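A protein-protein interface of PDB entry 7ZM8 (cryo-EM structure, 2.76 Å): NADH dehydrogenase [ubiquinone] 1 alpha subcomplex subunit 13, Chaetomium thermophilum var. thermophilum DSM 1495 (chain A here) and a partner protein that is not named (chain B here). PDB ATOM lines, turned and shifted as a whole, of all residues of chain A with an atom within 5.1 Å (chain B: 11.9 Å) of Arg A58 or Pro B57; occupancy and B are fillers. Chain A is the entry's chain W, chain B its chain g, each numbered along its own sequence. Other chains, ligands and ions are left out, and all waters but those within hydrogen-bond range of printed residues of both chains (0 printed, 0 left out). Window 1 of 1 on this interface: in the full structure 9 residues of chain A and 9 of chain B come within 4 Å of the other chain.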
ATOM      1  N   ASN A  54       4.417  20.500 -23.553  1.00  0.00           N
ATOM      2  CA  ASN A  54       4.831  20.627 -22.138  1.00  0.00           C
ATOM      3  C   ASN A  54       6.325  20.896 -22.060  1.00  0.00           C
ATOM      4  O   ASN A  54       6.762  21.430 -21.046  1.00  0.00           O
ATOM      5  CB  ASN A  54       4.359  19.417 -21.343  1.00  0.00           C
ATOM      6  CG  ASN A  54       2.874  19.400 -21.064  1.00  0.00           C
ATOM      7  OD1 ASN A  54       2.147  20.300 -21.465  1.00  0.00           O
ATOM      8  ND2 ASN A  54       2.410  18.375 -20.372  1.00  0.00           N
ATOM      9  N   GLU A  55       7.060  20.546 -23.106  1.00  0.00           N
ATOM     10  CA  GLU A  55       8.515  20.805 -23.163  1.00  0.00           C
ATOM     11  C   GLU A  55       8.757  22.185 -23.782  1.00  0.00           C
ATOM     12  O   GLU A  55       9.777  22.802 -23.479  1.00  0.00           O
ATOM     13  CB  GLU A  55       9.182  19.607 -23.841  1.00  0.00           C
ATOM     14  CG  GLU A  55       9.151  18.355 -22.989  1.00  0.00           C
ATOM     15  CD  GLU A  55       9.511  18.584 -21.531  1.00  0.00           C
ATOM     16  OE1 GLU A  55       8.790  18.061 -20.657  1.00  0.00           O
ATOM     17  OE2 GLU A  55      10.522  19.268 -21.273  1.00  0.00           O
ATOM     18  N   LEU A  56       7.853  22.653 -24.624  1.00  0.00           N
ATOM     19  CA  LEU A  56       7.899  24.044 -25.130  1.00  0.00           C
ATOM     20  C   LEU A  56       7.597  24.998 -23.985  1.00  0.00           C
ATOM     21  O   LEU A  56       8.192  26.067 -23.938  1.00  0.00           O
ATOM     22  CB  LEU A  56       6.897  24.181 -26.278  1.00  0.00           C
ATOM     23  CG  LEU A  56       7.294  23.519 -27.591  1.00  0.00           C
ATOM     24  CD1 LEU A  56       6.152  23.606 -28.584  1.00  0.00           C
ATOM     25  CD2 LEU A  56       8.553  24.151 -28.152  1.00  0.00           C
ATOM     26  N   ALA A  57       6.683  24.616 -23.109  1.00  0.00           N
ATOM     27  CA  ALA A  57       6.337  25.419 -21.923  1.00  0.00           C
ATOM     28  C   ALA A  57       7.533  25.501 -20.968  1.00  0.00           C
ATOM     29  O   ALA A  57       7.718  26.562 -20.364  1.00  0.00           O
ATOM     30  CB  ALA A  57       5.091  24.876 -21.276  1.00  0.00           C
ATOM     31  N   ARG A  58       8.302  24.428 -20.829  1.00  0.00           N
ATOM     32  CA  ARG A  58       9.497  24.423 -19.960  1.00  0.00           C
ATOM     33  C   ARG A  58      10.504  25.439 -20.487  1.00  0.00           C
ATOM     34  O   ARG A  58      11.113  26.120 -19.664  1.00  0.00           O
ATOM     35  CB  ARG A  58      10.143  23.039 -19.929  1.00  0.00           C
ATOM     36  CG  ARG A  58      11.246  22.900 -18.891  1.00  0.00           C
ATOM     37  CD  ARG A  58      11.863  21.517 -18.872  1.00  0.00           C
ATOM     38  NE  ARG A  58      10.855  20.486 -18.704  1.00  0.00           N
ATOM     39  CZ  ARG A  58      10.417  20.046 -17.533  1.00  0.00           C
ATOM     40  NH1 ARG A  58       9.493  19.104 -17.487  1.00  0.00           N
ATOM     41  NH2 ARG A  58      10.900  20.548 -16.414  1.00  0.00           N
ATOM     42  N   GLU A  59      10.629  25.591 -21.799  1.00  0.00           N
ATOM     43  CA  GLU A  59      11.663  26.480 -22.363  1.00  0.00           C
ATOM     44  C   GLU A  59      11.155  27.913 -22.282  1.00  0.00           C
ATOM     45  O   GLU A  59      11.964  28.808 -22.062  1.00  0.00           O
ATOM     46  CB  GLU A  59      11.811  26.147 -23.840  1.00  0.00           C
ATOM     47  CG  GLU A  59      12.771  27.041 -24.594  1.00  0.00           C
ATOM     48  CD  GLU A  59      12.846  26.729 -26.074  1.00  0.00           C
ATOM     49  OE1 GLU A  59      11.984  25.975 -26.555  1.00  0.00           O
ATOM     50  OE2 GLU A  59      13.766  27.235 -26.739  1.00  0.00           O
ATOM     51  N   LYS A  60       9.852  28.104 -22.403  1.00  0.00           N
ATOM     52  CA  LYS A  60       9.262  29.447 -22.248  1.00  0.00           C
ATOM     53  C   LYS A  60       9.459  29.937 -20.820  1.00  0.00           C
ATOM     54  O   LYS A  60       9.754  31.125 -20.650  1.00  0.00           O
ATOM     55  CB  LYS A  60       7.779  29.398 -22.596  1.00  0.00           C
ATOM     56  CG  LYS A  60       7.126  30.756 -22.793  1.00  0.00           C
ATOM     57  CD  LYS A  60       5.629  30.721 -22.700  1.00  0.00           C
ATOM     58  CE  LYS A  60       4.974  31.601 -23.739  1.00  0.00           C
ATOM     59  NZ  LYS A  60       4.873  30.937 -25.060  1.00  0.00           N
ATOM     60  N   MET A  61       9.305  29.070 -19.834  1.00  0.00           N
ATOM     61  CA  MET A  61       9.392  29.504 -18.424  1.00  0.00           C
ATOM     62  C   MET A  61      10.833  29.878 -18.113  1.00  0.00           C
ATOM     63  O   MET A  61      11.036  30.937 -17.545  1.00  0.00           O
ATOM     64  CB  MET A  61       8.814  28.460 -17.461  1.00  0.00           C
ATOM     65  CG  MET A  61       7.300  28.335 -17.539  1.00  0.00           C
ATOM     66  SD  MET A  61       6.383  29.821 -17.030  1.00  0.00           S
ATOM     67  CE  MET A  61       5.805  30.435 -18.612  1.00  0.00           C
ATOM     68  N   TRP A  62      11.786  29.028 -18.481  1.00  0.00           N
ATOM     69  CA  TRP A  62      13.226  29.264 -18.226  1.00  0.00           C
ATOM     70  C   TRP A  62      13.681  30.528 -18.937  1.00  0.00           C
ATOM     71  O   TRP A  62      14.543  31.210 -18.392  1.00  0.00           O
ATOM     72  CB  TRP A  62      14.017  28.013 -18.609  1.00  0.00           C
ATOM     73  CG  TRP A  62      13.927  26.972 -17.538  1.00  0.00           C
ATOM     74  CD1 TRP A  62      13.256  25.786 -17.587  1.00  0.00           C
ATOM     75  CD2 TRP A  62      14.484  27.061 -16.217  1.00  0.00           C
ATOM     76  NE1 TRP A  62      13.382  25.119 -16.400  1.00  0.00           N
ATOM     77  CE2 TRP A  62      14.126  25.878 -15.539  1.00  0.00           C
ATOM     78  CE3 TRP A  62      15.264  28.011 -15.552  1.00  0.00           C
ATOM     79  CZ2 TRP A  62      14.518  25.628 -14.228  1.00  0.00           C
ATOM     80  CZ3 TRP A  62      15.651  27.763 -14.258  1.00  0.00           C
ATOM     81  CH2 TRP A  62      15.283  26.588 -13.607  1.00  0.00           C
ATOM     82  N   ARG B  47       4.028   1.493 -17.986  1.00  0.00           N
ATOM     83  CA  ARG B  47       4.836   2.614 -18.543  1.00  0.00           C
ATOM     84  C   ARG B  47       6.210   2.648 -17.875  1.00  0.00           C
ATOM     85  O   ARG B  47       7.202   2.808 -18.588  1.00  0.00           O
ATOM     86  CB  ARG B  47       4.145   3.966 -18.333  1.00  0.00           C
ATOM     87  CG  ARG B  47       3.260   4.402 -19.489  1.00  0.00           C
ATOM     88  CD  ARG B  47       2.721   5.812 -19.378  1.00  0.00           C
ATOM     89  NE  ARG B  47       3.730   6.856 -19.266  1.00  0.00           N
ATOM     90  CZ  ARG B  47       3.872   7.669 -18.225  1.00  0.00           C
ATOM     91  NH1 ARG B  47       4.825   8.583 -18.230  1.00  0.00           N
ATOM     92  NH2 ARG B  47       3.066   7.571 -17.186  1.00  0.00           N
ATOM     93  N   VAL B  53       9.341   7.546 -18.468  1.00  0.00           N
ATOM     94  CA  VAL B  53       9.313   8.276 -17.166  1.00  0.00           C
ATOM     95  C   VAL B  53       8.386   9.481 -17.236  1.00  0.00           C
ATOM     96  O   VAL B  53       8.109   9.946 -18.345  1.00  0.00           O
ATOM     97  CB  VAL B  53      10.726   8.671 -16.698  1.00  0.00           C
ATOM     98  CG1 VAL B  53      11.645   7.463 -16.615  1.00  0.00           C
ATOM     99  CG2 VAL B  53      11.342   9.754 -17.569  1.00  0.00           C
ATOM    100  N   ASP B  54       7.873   9.918 -16.090  1.00  0.00           N
ATOM    101  CA  ASP B  54       7.069  11.164 -16.058  1.00  0.00           C
ATOM    102  C   ASP B  54       8.009  12.353 -16.221  1.00  0.00           C
ATOM    103  O   ASP B  54       9.155  12.271 -15.749  1.00  0.00           O
ATOM    104  CB  ASP B  54       6.305  11.334 -14.747  1.00  0.00           C
ATOM    105  CG  ASP B  54       5.187  10.323 -14.559  1.00  0.00           C
ATOM    106  OD1 ASP B  54       4.305  10.579 -13.717  1.00  0.00           O
ATOM    107  OD2 ASP B  54       5.209   9.287 -15.250  1.00  0.00           O
ATOM    108  N   ALA B  55       7.538  13.405 -16.874  1.00  0.00           N
ATOM    109  CA  ALA B  55       8.333  14.636 -17.000  1.00  0.00           C
ATOM    110  C   ALA B  55       8.395  15.305 -15.630  1.00  0.00           C
ATOM    111  O   ALA B  55       7.428  15.150 -14.868  1.00  0.00           O
ATOM    112  CB  ALA B  55       7.649  15.513 -18.007  1.00  0.00           C
ATOM    113  N   ALA B  56       9.482  16.012 -15.316  1.00  0.00           N
ATOM    114  CA  ALA B  56       9.527  16.779 -14.051  1.00  0.00           C
ATOM    115  C   ALA B  56       8.499  17.897 -14.174  1.00  0.00           C
ATOM    116  O   ALA B  56       8.205  18.287 -15.314  1.00  0.00           O
ATOM    117  CB  ALA B  56      10.908  17.336 -13.836  1.00  0.00           C
ATOM    118  N   PRO B  57       7.933  18.441 -13.077  1.00  0.00           N
ATOM    119  CA  PRO B  57       7.010  19.558 -13.220  1.00  0.00           C
ATOM    120  C   PRO B  57       7.754  20.762 -13.821  1.00  0.00           C
ATOM    121  O   PRO B  57       8.925  20.939 -13.556  1.00  0.00           O
ATOM    122  CB  PRO B  57       6.477  19.753 -11.797  1.00  0.00           C
ATOM    123  CG  PRO B  57       7.556  19.172 -10.909  1.00  0.00           C
ATOM    124  CD  PRO B  57       8.123  18.009 -11.694  1.00  0.00           C
ATOM    125  N   ILE B  58       7.069  21.530 -14.667  1.00  0.00           N
ATOM    126  CA  ILE B  58       7.703  22.736 -15.267  1.00  0.00           C
ATOM    127  C   ILE B  58       7.765  23.849 -14.206  1.00  0.00           C
ATOM    128  O   ILE B  58       6.924  23.802 -13.291  1.00  0.00           O
ATOM    129  CB  ILE B  58       7.009  23.191 -16.569  1.00  0.00           C
ATOM    130  CG1 ILE B  58       5.652  23.850 -16.309  1.00  0.00           C
ATOM    131  CG2 ILE B  58       6.918  22.049 -17.568  1.00  0.00           C
ATOM    132  CD1 ILE B  58       5.268  24.879 -17.344  1.00  0.00           C
ATOM    133  N   PRO B  59       8.712  24.828 -14.239  1.00  0.00           N
ATOM    134  CA  PRO B  59       8.680  25.901 -13.243  1.00  0.00           C
ATOM    135  C   PRO B  59       7.501  26.892 -13.339  1.00  0.00           C
ATOM    136  O   PRO B  59       7.220  27.364 -14.398  1.00  0.00           O
ATOM    137  CB  PRO B  59      10.041  26.560 -13.466  1.00  0.00           C
ATOM    138  CG  PRO B  59      10.373  26.298 -14.913  1.00  0.00           C
ATOM    139  CD  PRO B  59       9.824  24.919 -15.183  1.00  0.00           C
ATOM    140  N   LEU B  60       6.853  27.200 -12.217  1.00  0.00           N
ATOM    141  CA  LEU B  60       5.677  28.112 -12.201  1.00  0.00           C
ATOM    142  C   LEU B  60       5.944  29.222 -11.189  1.00  0.00           C
ATOM    143  O   LEU B  60       5.044  30.031 -10.983  1.00  0.00           O
ATOM    144  CB  LEU B  60       4.409  27.329 -11.860  1.00  0.00           C
ATOM    145  CG  LEU B  60       3.913  26.368 -12.937  1.00  0.00           C
ATOM    146  CD1 LEU B  60       2.740  25.547 -12.430  1.00  0.00           C
ATOM    147  CD2 LEU B  60       3.529  27.116 -14.203  1.00  0.00           C
ATOM    148  N   THR B  61       7.130  29.239 -10.591  1.00  0.00           N
ATOM    149  CA  THR B  61       7.576  30.308  -9.669  1.00  0.00           C
ATOM    150  C   THR B  61       9.057  30.464  -9.992  1.00  0.00           C
ATOM    151  O   THR B  61       9.613  29.507 -10.543  1.00  0.00           O
ATOM    152  CB  THR B  61       7.300  29.946  -8.202  1.00  0.00           C
ATOM    153  OG1 THR B  61       7.323  31.116  -7.390  1.00  0.00           O
ATOM    154  CG2 THR B  61       8.253  28.912  -7.643  1.00  0.00           C
ATOM    155  N   TYR B  62       9.672  31.605  -9.696  1.00  0.00           N
ATOM    156  CA  TYR B  62      11.136  31.698  -9.916  1.00  0.00           C
ATOM    157  C   TYR B  62      11.812  30.617  -9.087  1.00  0.00           C
ATOM    158  O   TYR B  62      11.520  30.479  -7.893  1.00  0.00           O
ATOM    159  CB  TYR B  62      11.707  33.062  -9.529  1.00  0.00           C
ATOM    160  CG  TYR B  62      13.173  33.228  -9.830  1.00  0.00           C
ATOM    161  CD1 TYR B  62      14.138  32.746  -8.965  1.00  0.00           C
ATOM    162  CD2 TYR B  62      13.594  33.854 -10.988  1.00  0.00           C
ATOM    163  CE1 TYR B  62      15.487  32.876  -9.243  1.00  0.00           C
ATOM    164  CE2 TYR B  62      14.937  34.000 -11.278  1.00  0.00           C
ATOM    165  CZ  TYR B  62      15.886  33.506 -10.406  1.00  0.00           C
ATOM    166  OH  TYR B  62      17.207  33.657 -10.697  1.00  0.00           O
ATOM    167  N   PRO B  63      12.775  29.880  -9.672  1.00  0.00           N
ATOM    168  CA  PRO B  63      13.396  28.770  -8.969  1.00  0.00           C
ATOM    169  C   PRO B  63      14.511  29.241  -8.036  1.00  0.00           C
ATOM    170  O   PRO B  63      15.652  29.240  -8.444  1.00  0.00           O
ATOM    171  CB  PRO B  63      13.995  27.981 -10.123  1.00  0.00           C
ATOM    172  CG  PRO B  63      14.341  29.016 -11.163  1.00  0.00           C
ATOM    173  CD  PRO B  63      13.268  30.064 -11.029  1.00  0.00           C
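Asn A54 touches Ile B58.
CB of Ala B55 touches OE1 of Glu A55, at 3.8 Å.
CD1 of Ile B58 touches CB of Ala A57 (3.9 Å).
Ile B58 touches Arg A58 (CG2 to NH1, 3.9 Å).
Trp A62 touches Pro B59 (NE1 to CG, 3.6 Å).
Trp A62 touches Pro B63.
Of chain A, only Arg A58 comes within 4 Å of Pro B57.
Of chain B, only Ile B58 comes within 4 Å of Asn A54.
Glu A55 touches just one residue of chain B: Ala B55.
Of chain B, only Ile B58 (3.9 Å) comes within 4 Å of Ala A57.
No residue of chain B comes within 4 Å of Glu A59.
Printed residues of chain B within 4 Å of Trp A62: Pro B59 (3.6 Å) and Pro B63 (3.6 Å).
Printed residues of chain A within 4 Å of Pro B59: Met A61 and Trp A62.
Printed residues of chain A within 4 Å of Ile B58: Asn A54 (3.5 Å), Ala A57 (3.9 Å) and Arg A58 (3.9 Å).
Printed residues of chain A within 4 Å of Pro B63: Trp A62.
Of the printed residues of chain A, Ala B56 touches Arg A58 (2.7 Å).
The nearest printed residue of chain A that does not touch Pro B57 is Trp A62 (6.7 Å).
OE2 of Glu A55 is in salt-bridge range of NE of Arg A58 (2.9 Å).
Of the 12 printed residues of chain B, 6 touch a printed residue of chain A.
Hydrophobic or aromatic side chains of chain B within 4 Å of the printed part of chain A: Ala B55, Ile B58, Pro B59 and Pro B63.
Along chain B the printed residues that touch a printed residue of chain A span positions 55 to 63.
Along chain A the printed residues that touch a printed residue of chain B span positions 54 to 62.
O of Ala B56 is in hydrogen-bond range of NH1 of Arg A58, at 2.7 Å.
The guanidinium group (NH2) of Arg A58 is in hydrogen-bond range of the backbone carbonyl oxygen (O) of Pro B57 (3.5 Å).
The side-chain sulfur of Met A61 sits close to the backbone carbonyl oxygen of Pro B59, 3.7 Å away.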
